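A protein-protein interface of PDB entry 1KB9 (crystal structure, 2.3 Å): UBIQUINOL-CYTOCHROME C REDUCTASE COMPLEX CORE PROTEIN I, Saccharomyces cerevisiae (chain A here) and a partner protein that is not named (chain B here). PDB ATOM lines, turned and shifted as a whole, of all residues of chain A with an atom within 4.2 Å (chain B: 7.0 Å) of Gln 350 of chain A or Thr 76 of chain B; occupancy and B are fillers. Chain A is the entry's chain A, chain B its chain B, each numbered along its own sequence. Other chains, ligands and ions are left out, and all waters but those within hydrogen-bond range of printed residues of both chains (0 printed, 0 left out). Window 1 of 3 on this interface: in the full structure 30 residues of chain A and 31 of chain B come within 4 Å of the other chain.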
ATOM      1  N   LEU A 346      25.999  -5.585  -8.924  1.00  0.00           N
ATOM      2  CA  LEU A 346      25.679  -4.399  -9.701  1.00  0.00           C
ATOM      3  C   LEU A 346      25.118  -4.747 -11.072  1.00  0.00           C
ATOM      4  O   LEU A 346      24.165  -4.119 -11.527  1.00  0.00           O
ATOM      5  CB  LEU A 346      26.916  -3.514  -9.858  1.00  0.00           C
ATOM      6  CG  LEU A 346      26.749  -2.255 -10.714  1.00  0.00           C
ATOM      7  CD1 LEU A 346      25.827  -1.268 -10.018  1.00  0.00           C
ATOM      8  CD2 LEU A 346      28.104  -1.623 -10.974  1.00  0.00           C
ATOM      9  N   GLN A 347      25.699  -5.748 -11.729  1.00  0.00           N
ATOM     10  CA  GLN A 347      25.230  -6.130 -13.057  1.00  0.00           C
ATOM     11  C   GLN A 347      23.950  -6.943 -12.988  1.00  0.00           C
ATOM     12  O   GLN A 347      23.069  -6.776 -13.823  1.00  0.00           O
ATOM     13  CB  GLN A 347      26.305  -6.895 -13.847  1.00  0.00           C
ATOM     14  CG  GLN A 347      26.493  -8.362 -13.456  1.00  0.00           C
ATOM     15  CD  GLN A 347      26.654  -9.279 -14.663  1.00  0.00           C
ATOM     16  OE1 GLN A 347      26.111  -9.012 -15.739  1.00  0.00           O
ATOM     17  NE2 GLN A 347      27.393 -10.372 -14.485  1.00  0.00           N
ATOM     18  N   LEU A 348      23.854  -7.816 -11.991  1.00  0.00           N
ATOM     19  CA  LEU A 348      22.676  -8.654 -11.813  1.00  0.00           C
ATOM     20  C   LEU A 348      21.488  -7.775 -11.427  1.00  0.00           C
ATOM     21  O   LEU A 348      20.341  -8.077 -11.761  1.00  0.00           O
ATOM     22  CB  LEU A 348      22.940  -9.703 -10.738  1.00  0.00           C
ATOM     23  CG  LEU A 348      22.377 -11.095 -11.011  1.00  0.00           C
ATOM     24  CD1 LEU A 348      22.820 -11.572 -12.386  1.00  0.00           C
ATOM     25  CD2 LEU A 348      22.845 -12.055  -9.930  1.00  0.00           C
ATOM     26  N   GLY A 349      21.783  -6.684 -10.724  1.00  0.00           N
ATOM     27  CA  GLY A 349      20.754  -5.747 -10.328  1.00  0.00           C
ATOM     28  C   GLY A 349      20.271  -5.001 -11.554  1.00  0.00           C
ATOM     29  O   GLY A 349      19.084  -5.026 -11.863  1.00  0.00           O
ATOM     30  N   GLN A 350      21.198  -4.387 -12.287  1.00  0.00           N
ATOM     31  CA  GLN A 350      20.865  -3.633 -13.497  1.00  0.00           C
ATOM     32  C   GLN A 350      20.068  -4.431 -14.536  1.00  0.00           C
ATOM     33  O   GLN A 350      19.431  -3.847 -15.414  1.00  0.00           O
ATOM     34  CB  GLN A 350      22.130  -3.087 -14.153  1.00  0.00           C
ATOM     35  CG  GLN A 350      22.770  -1.924 -13.434  1.00  0.00           C
ATOM     36  CD  GLN A 350      24.006  -1.421 -14.155  1.00  0.00           C
ATOM     37  OE1 GLN A 350      25.097  -1.966 -13.989  1.00  0.00           O
ATOM     38  NE2 GLN A 350      23.838  -0.387 -14.971  1.00  0.00           N
ATOM     39  N   LEU A 351      20.145  -5.757 -14.460  1.00  0.00           N
ATOM     40  CA  LEU A 351      19.416  -6.624 -15.382  1.00  0.00           C
ATOM     41  C   LEU A 351      18.010  -6.887 -14.861  1.00  0.00           C
ATOM     42  O   LEU A 351      17.024  -6.566 -15.524  1.00  0.00           O
ATOM     43  CB  LEU A 351      20.144  -7.961 -15.573  1.00  0.00           C
ATOM     44  CG  LEU A 351      20.947  -8.159 -16.864  1.00  0.00           C
ATOM     45  CD1 LEU A 351      21.697  -9.486 -16.805  1.00  0.00           C
ATOM     46  CD2 LEU A 351      20.021  -8.119 -18.073  1.00  0.00           C
ATOM     47  N   TYR A 352      17.935  -7.457 -13.660  1.00  0.00           N
ATOM     48  CA  TYR A 352      16.666  -7.785 -13.022  1.00  0.00           C
ATOM     49  C   TYR A 352      15.762  -6.584 -12.765  1.00  0.00           C
ATOM     50  O   TYR A 352      14.536  -6.716 -12.779  1.00  0.00           O
ATOM     51  CB  TYR A 352      16.903  -8.551 -11.718  1.00  0.00           C
ATOM     52  CG  TYR A 352      17.206 -10.023 -11.907  1.00  0.00           C
ATOM     53  CD1 TYR A 352      16.657 -10.979 -11.052  1.00  0.00           C
ATOM     54  CD2 TYR A 352      18.039 -10.463 -12.938  1.00  0.00           C
ATOM     55  CE1 TYR A 352      16.927 -12.339 -11.219  1.00  0.00           C
ATOM     56  CE2 TYR A 352      18.316 -11.820 -13.116  1.00  0.00           C
ATOM     57  CZ  TYR A 352      17.757 -12.751 -12.253  1.00  0.00           C
ATOM     58  OH  TYR A 352      18.025 -14.092 -12.421  1.00  0.00           O
ATOM     59  N   SER A 354      15.378  -3.152 -14.420  1.00  0.00           N
ATOM     60  CA  SER A 354      15.522  -2.088 -15.400  1.00  0.00           C
ATOM     61  C   SER A 354      14.166  -1.383 -15.471  1.00  0.00           C
ATOM     62  O   SER A 354      13.170  -1.875 -14.922  1.00  0.00           O
ATOM     63  CB  SER A 354      15.872  -2.674 -16.770  1.00  0.00           C
ATOM     64  OG  SER A 354      16.075  -1.646 -17.726  1.00  0.00           O
ATOM     65  N   ILE B  12      19.217  -1.232  -6.515  1.00  0.00           N
ATOM     66  CA  ILE B  12      20.130  -0.409  -7.304  1.00  0.00           C
ATOM     67  C   ILE B  12      19.667   1.040  -7.400  1.00  0.00           C
ATOM     68  O   ILE B  12      18.576   1.317  -7.893  1.00  0.00           O
ATOM     69  CB  ILE B  12      20.294  -0.969  -8.752  1.00  0.00           C
ATOM     70  CG1 ILE B  12      20.834  -2.401  -8.718  1.00  0.00           C
ATOM     71  CG2 ILE B  12      21.207  -0.073  -9.577  1.00  0.00           C
ATOM     72  CD1 ILE B  12      22.215  -2.531  -8.120  1.00  0.00           C
ATOM     73  N   SER B  13      20.505   1.960  -6.933  1.00  0.00           N
ATOM     74  CA  SER B  13      20.196   3.386  -6.989  1.00  0.00           C
ATOM     75  C   SER B  13      21.004   4.013  -8.115  1.00  0.00           C
ATOM     76  O   SER B  13      21.968   3.421  -8.596  1.00  0.00           O
ATOM     77  CB  SER B  13      20.540   4.063  -5.662  1.00  0.00           C
ATOM     78  OG  SER B  13      19.853   3.453  -4.582  1.00  0.00           O
ATOM     79  N   THR B  14      20.614   5.209  -8.543  1.00  0.00           N
ATOM     80  CA  THR B  14      21.327   5.883  -9.618  1.00  0.00           C
ATOM     81  C   THR B  14      21.319   7.407  -9.525  1.00  0.00           C
ATOM     82  O   THR B  14      20.358   8.069  -9.916  1.00  0.00           O
ATOM     83  CB  THR B  14      20.852   5.394 -11.027  1.00  0.00           C
ATOM     84  OG1 THR B  14      21.148   6.385 -12.021  1.00  0.00           O
ATOM     85  CG2 THR B  14      19.365   5.084 -11.036  1.00  0.00           C
ATOM     86  N   LEU B  15      22.414   7.946  -9.000  1.00  0.00           N
ATOM     87  CA  LEU B  15      22.602   9.385  -8.848  1.00  0.00           C
ATOM     88  C   LEU B  15      22.921   9.956 -10.232  1.00  0.00           C
ATOM     89  O   LEU B  15      23.493   9.265 -11.067  1.00  0.00           O
ATOM     90  CB  LEU B  15      23.778   9.639  -7.899  1.00  0.00           C
ATOM     91  CG  LEU B  15      23.759  10.808  -6.909  1.00  0.00           C
ATOM     92  CD1 LEU B  15      23.612  12.131  -7.639  1.00  0.00           C
ATOM     93  CD2 LEU B  15      22.631  10.611  -5.905  1.00  0.00           C
ATOM     94  N   GLY B  59      30.861  -1.484  -5.459  1.00  0.00           N
ATOM     95  CA  GLY B  59      29.869  -2.058  -6.340  1.00  0.00           C
ATOM     96  C   GLY B  59      29.108  -0.992  -7.088  1.00  0.00           C
ATOM     97  O   GLY B  59      27.882  -0.955  -7.030  1.00  0.00           O
ATOM     98  N   GLY B  60      29.828  -0.128  -7.795  1.00  0.00           N
ATOM     99  CA  GLY B  60      29.187   0.931  -8.553  1.00  0.00           C
ATOM    100  C   GLY B  60      30.083   1.476  -9.647  1.00  0.00           C
ATOM    101  O   GLY B  60      31.306   1.397  -9.540  1.00  0.00           O
ATOM    102  N   THR B  61      29.482   2.018 -10.705  1.00  0.00           N
ATOM    103  CA  THR B  61      30.248   2.576 -11.818  1.00  0.00           C
ATOM    104  C   THR B  61      29.857   4.018 -12.118  1.00  0.00           C
ATOM    105  O   THR B  61      28.826   4.504 -11.659  1.00  0.00           O
ATOM    106  CB  THR B  61      30.077   1.744 -13.121  1.00  0.00           C
ATOM    107  OG1 THR B  61      28.707   1.778 -13.544  1.00  0.00           O
ATOM    108  CG2 THR B  61      30.504   0.297 -12.902  1.00  0.00           C
ATOM    109  N   PHE B  62      30.698   4.693 -12.893  1.00  0.00           N
ATOM    110  CA  PHE B  62      30.457   6.074 -13.282  1.00  0.00           C
ATOM    111  C   PHE B  62      30.347   6.149 -14.798  1.00  0.00           C
ATOM    112  O   PHE B  62      30.721   5.208 -15.498  1.00  0.00           O
ATOM    113  CB  PHE B  62      31.589   6.974 -12.788  1.00  0.00           C
ATOM    114  CG  PHE B  62      31.674   7.074 -11.291  1.00  0.00           C
ATOM    115  CD1 PHE B  62      32.439   6.172 -10.562  1.00  0.00           C
ATOM    116  CD2 PHE B  62      30.986   8.075 -10.607  1.00  0.00           C
ATOM    117  CE1 PHE B  62      32.521   6.264  -9.175  1.00  0.00           C
ATOM    118  CE2 PHE B  62      31.061   8.178  -9.222  1.00  0.00           C
ATOM    119  CZ  PHE B  62      31.832   7.269  -8.503  1.00  0.00           C
ATOM    120  N   LYS B  63      29.850   7.276 -15.298  1.00  0.00           N
ATOM    121  CA  LYS B  63      29.664   7.478 -16.731  1.00  0.00           C
ATOM    122  C   LYS B  63      29.306   8.941 -16.977  1.00  0.00           C
ATOM    123  O   LYS B  63      28.546   9.532 -16.213  1.00  0.00           O
ATOM    124  CB  LYS B  63      28.539   6.561 -17.235  1.00  0.00           C
ATOM    125  CG  LYS B  63      28.126   6.759 -18.689  1.00  0.00           C
ATOM    126  CD  LYS B  63      29.281   6.520 -19.649  1.00  0.00           C
ATOM    127  CE  LYS B  63      28.896   6.883 -21.081  1.00  0.00           C
ATOM    128  NZ  LYS B  63      30.050   6.727 -22.018  1.00  0.00           N
ATOM    129  N   LYS B  74      26.327  10.653 -14.484  1.00  0.00           N
ATOM    130  CA  LYS B  74      25.540   9.624 -13.806  1.00  0.00           C
ATOM    131  C   LYS B  74      26.406   8.629 -13.034  1.00  0.00           C
ATOM    132  O   LYS B  74      27.575   8.431 -13.359  1.00  0.00           O
ATOM    133  CB  LYS B  74      24.675   8.895 -14.840  1.00  0.00           C
ATOM    134  CG  LYS B  74      23.687   7.880 -14.283  1.00  0.00           C
ATOM    135  CD  LYS B  74      22.940   7.190 -15.421  1.00  0.00           C
ATOM    136  CE  LYS B  74      22.087   6.034 -14.921  1.00  0.00           C
ATOM    137  NZ  LYS B  74      21.450   5.277 -16.041  1.00  0.00           N
ATOM    138  N   ALA B  75      25.823   8.004 -12.014  1.00  0.00           N
ATOM    139  CA  ALA B  75      26.529   7.026 -11.190  1.00  0.00           C
ATOM    140  C   ALA B  75      25.571   5.957 -10.683  1.00  0.00           C
ATOM    141  O   ALA B  75      24.711   6.227  -9.849  1.00  0.00           O
ATOM    142  CB  ALA B  75      27.210   7.713 -10.017  1.00  0.00           C
ATOM    143  N   THR B  76      25.731   4.742 -11.190  1.00  0.00           N
ATOM    144  CA  THR B  76      24.890   3.613 -10.811  1.00  0.00           C
ATOM    145  C   THR B  76      25.608   2.830  -9.718  1.00  0.00           C
ATOM    146  O   THR B  76      26.806   2.586  -9.828  1.00  0.00           O
ATOM    147  CB  THR B  76      24.651   2.719 -12.024  1.00  0.00           C
ATOM    148  OG1 THR B  76      24.254   3.536 -13.132  1.00  0.00           O
ATOM    149  CG2 THR B  76      23.571   1.697 -11.733  1.00  0.00           C
ATOM    150  N   PHE B  77      24.877   2.400  -8.691  1.00  0.00           N
ATOM    151  CA  PHE B  77      25.493   1.686  -7.570  1.00  0.00           C
ATOM    152  C   PHE B  77      24.494   0.979  -6.670  1.00  0.00           C
ATOM    153  O   PHE B  77      23.294   0.986  -6.930  1.00  0.00           O
ATOM    154  CB  PHE B  77      26.255   2.688  -6.707  1.00  0.00           C
ATOM    155  CG  PHE B  77      25.406   3.845  -6.241  1.00  0.00           C
ATOM    156  CD1 PHE B  77      24.779   3.814  -4.996  1.00  0.00           C
ATOM    157  CD2 PHE B  77      25.211   4.955  -7.060  1.00  0.00           C
ATOM    158  CE1 PHE B  77      23.966   4.873  -4.577  1.00  0.00           C
ATOM    159  CE2 PHE B  77      24.401   6.016  -6.649  1.00  0.00           C
ATOM    160  CZ  PHE B  77      23.777   5.974  -5.406  1.00  0.00           C
ATOM    161  N   LEU B  78      25.009   0.390  -5.593  1.00  0.00           N
ATOM    162  CA  LEU B  78      24.178  -0.295  -4.610  1.00  0.00           C
ATOM    163  C   LEU B  78      23.645   0.762  -3.638  1.00  0.00           C
ATOM    164  O   LEU B  78      24.413   1.543  -3.076  1.00  0.00           O
ATOM    165  CB  LEU B  78      24.985  -1.354  -3.853  1.00  0.00           C
ATOM    166  CG  LEU B  78      25.660  -2.454  -4.681  1.00  0.00           C
ATOM    167  CD1 LEU B  78      26.336  -3.453  -3.751  1.00  0.00           C
ATOM    168  CD2 LEU B  78      24.641  -3.155  -5.554  1.00  0.00           C
ATOM    169  N   TYR B  85      29.145   8.208  -3.617  1.00  0.00           N
ATOM    170  CA  TYR B  85      28.941   8.677  -4.981  1.00  0.00           C
ATOM    171  C   TYR B  85      28.548  10.145  -5.079  1.00  0.00           C
ATOM    172  O   TYR B  85      28.808  10.793  -6.100  1.00  0.00           O
ATOM    173  CB  TYR B  85      27.944   7.770  -5.701  1.00  0.00           C
ATOM    174  CG  TYR B  85      28.399   6.326  -5.706  1.00  0.00           C
ATOM    175  CD1 TYR B  85      28.121   5.490  -4.625  1.00  0.00           C
ATOM    176  CD2 TYR B  85      29.162   5.811  -6.760  1.00  0.00           C
ATOM    177  CE1 TYR B  85      28.595   4.179  -4.589  1.00  0.00           C
ATOM    178  CE2 TYR B  85      29.640   4.499  -6.733  1.00  0.00           C
ATOM    179  CZ  TYR B  85      29.352   3.692  -5.645  1.00  0.00           C
ATOM    180  OH  TYR B  85      29.816   2.399  -5.592  1.00  0.00           O
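The backbone NH (N) of Thr 61 of chain B sits at hydrogen-bond distance from the backbone carbonyl oxygen (O) of Thr 76 of chain B (2.9 Å). The backbone NH (N) of Ser 13 of chain B is in hydrogen-bond range of the backbone carbonyl oxygen (O) of Phe 77 of chain B (3.0 Å). N of Gly 60 of chain B lies within hydrogen-bond range of OH of Tyr 85 of chain B. O of Leu 346 of chain A lies close to OE1 of Gln 350 of chain A. The backbone NH (N) of Leu 78 of chain B is in hydrogen-bond range of the backbone carbonyl oxygen (O) of Gly 59 of chain B (3.5 Å).
Gln 350 of chain A touches one residue of chain B. Of the printed residues of chain A, Thr 76 of chain B touches Leu 346 and Gln 350. Gly 349 of chain A touches just one residue of chain B: Ile 12. Of the printed residues of chain A, Thr 61 of chain B touches Leu 346 (3.6 Å). Of the printed residues of chain A, Gly 60 of chain B touches Leu 346. Printed residues of chain B within 4 Å of Leu 346 of chain A: Gly 59 (3.6 Å), Gly 60 (3.7 Å), Thr 61 (3.6 Å), Thr 76 (3.98 Å) and Phe 77 (3.9 Å). Printed residues of chain A within 4 Å of Ile 12 of chain B: Gly 349. Ser 354 of chain A touches none of the printed residues of chain B.
Printed residues of chain A that touch a printed residue of chain B: Leu 346, Gly 349 and Gln 350. Hydrophobic or aromatic side chains of chain A within 4 Å of the printed part of chain B: Leu 346. Of the 15 printed residues of chain B, 6 touch a printed residue of chain A.
Among the printed residues, merely in contact across the chains: Leu 346 of chain A with Thr 61 of chain B (3.6 Å), Leu 346 of chain A with Gly 59 of chain B (3.6 Å), Leu 346 of chain A with Gly 60 of chain B (3.7 Å), Gly 349 of chain A with Ile 12 of chain B (3.7 Å), Leu 346 of chain A with Phe 77 of chain B (3.9 Å), Gln 350 of chain A with Thr 76 of chain B (3.9 Å) and Leu 346 of chain A with Thr 76 of chain B (3.98 Å).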
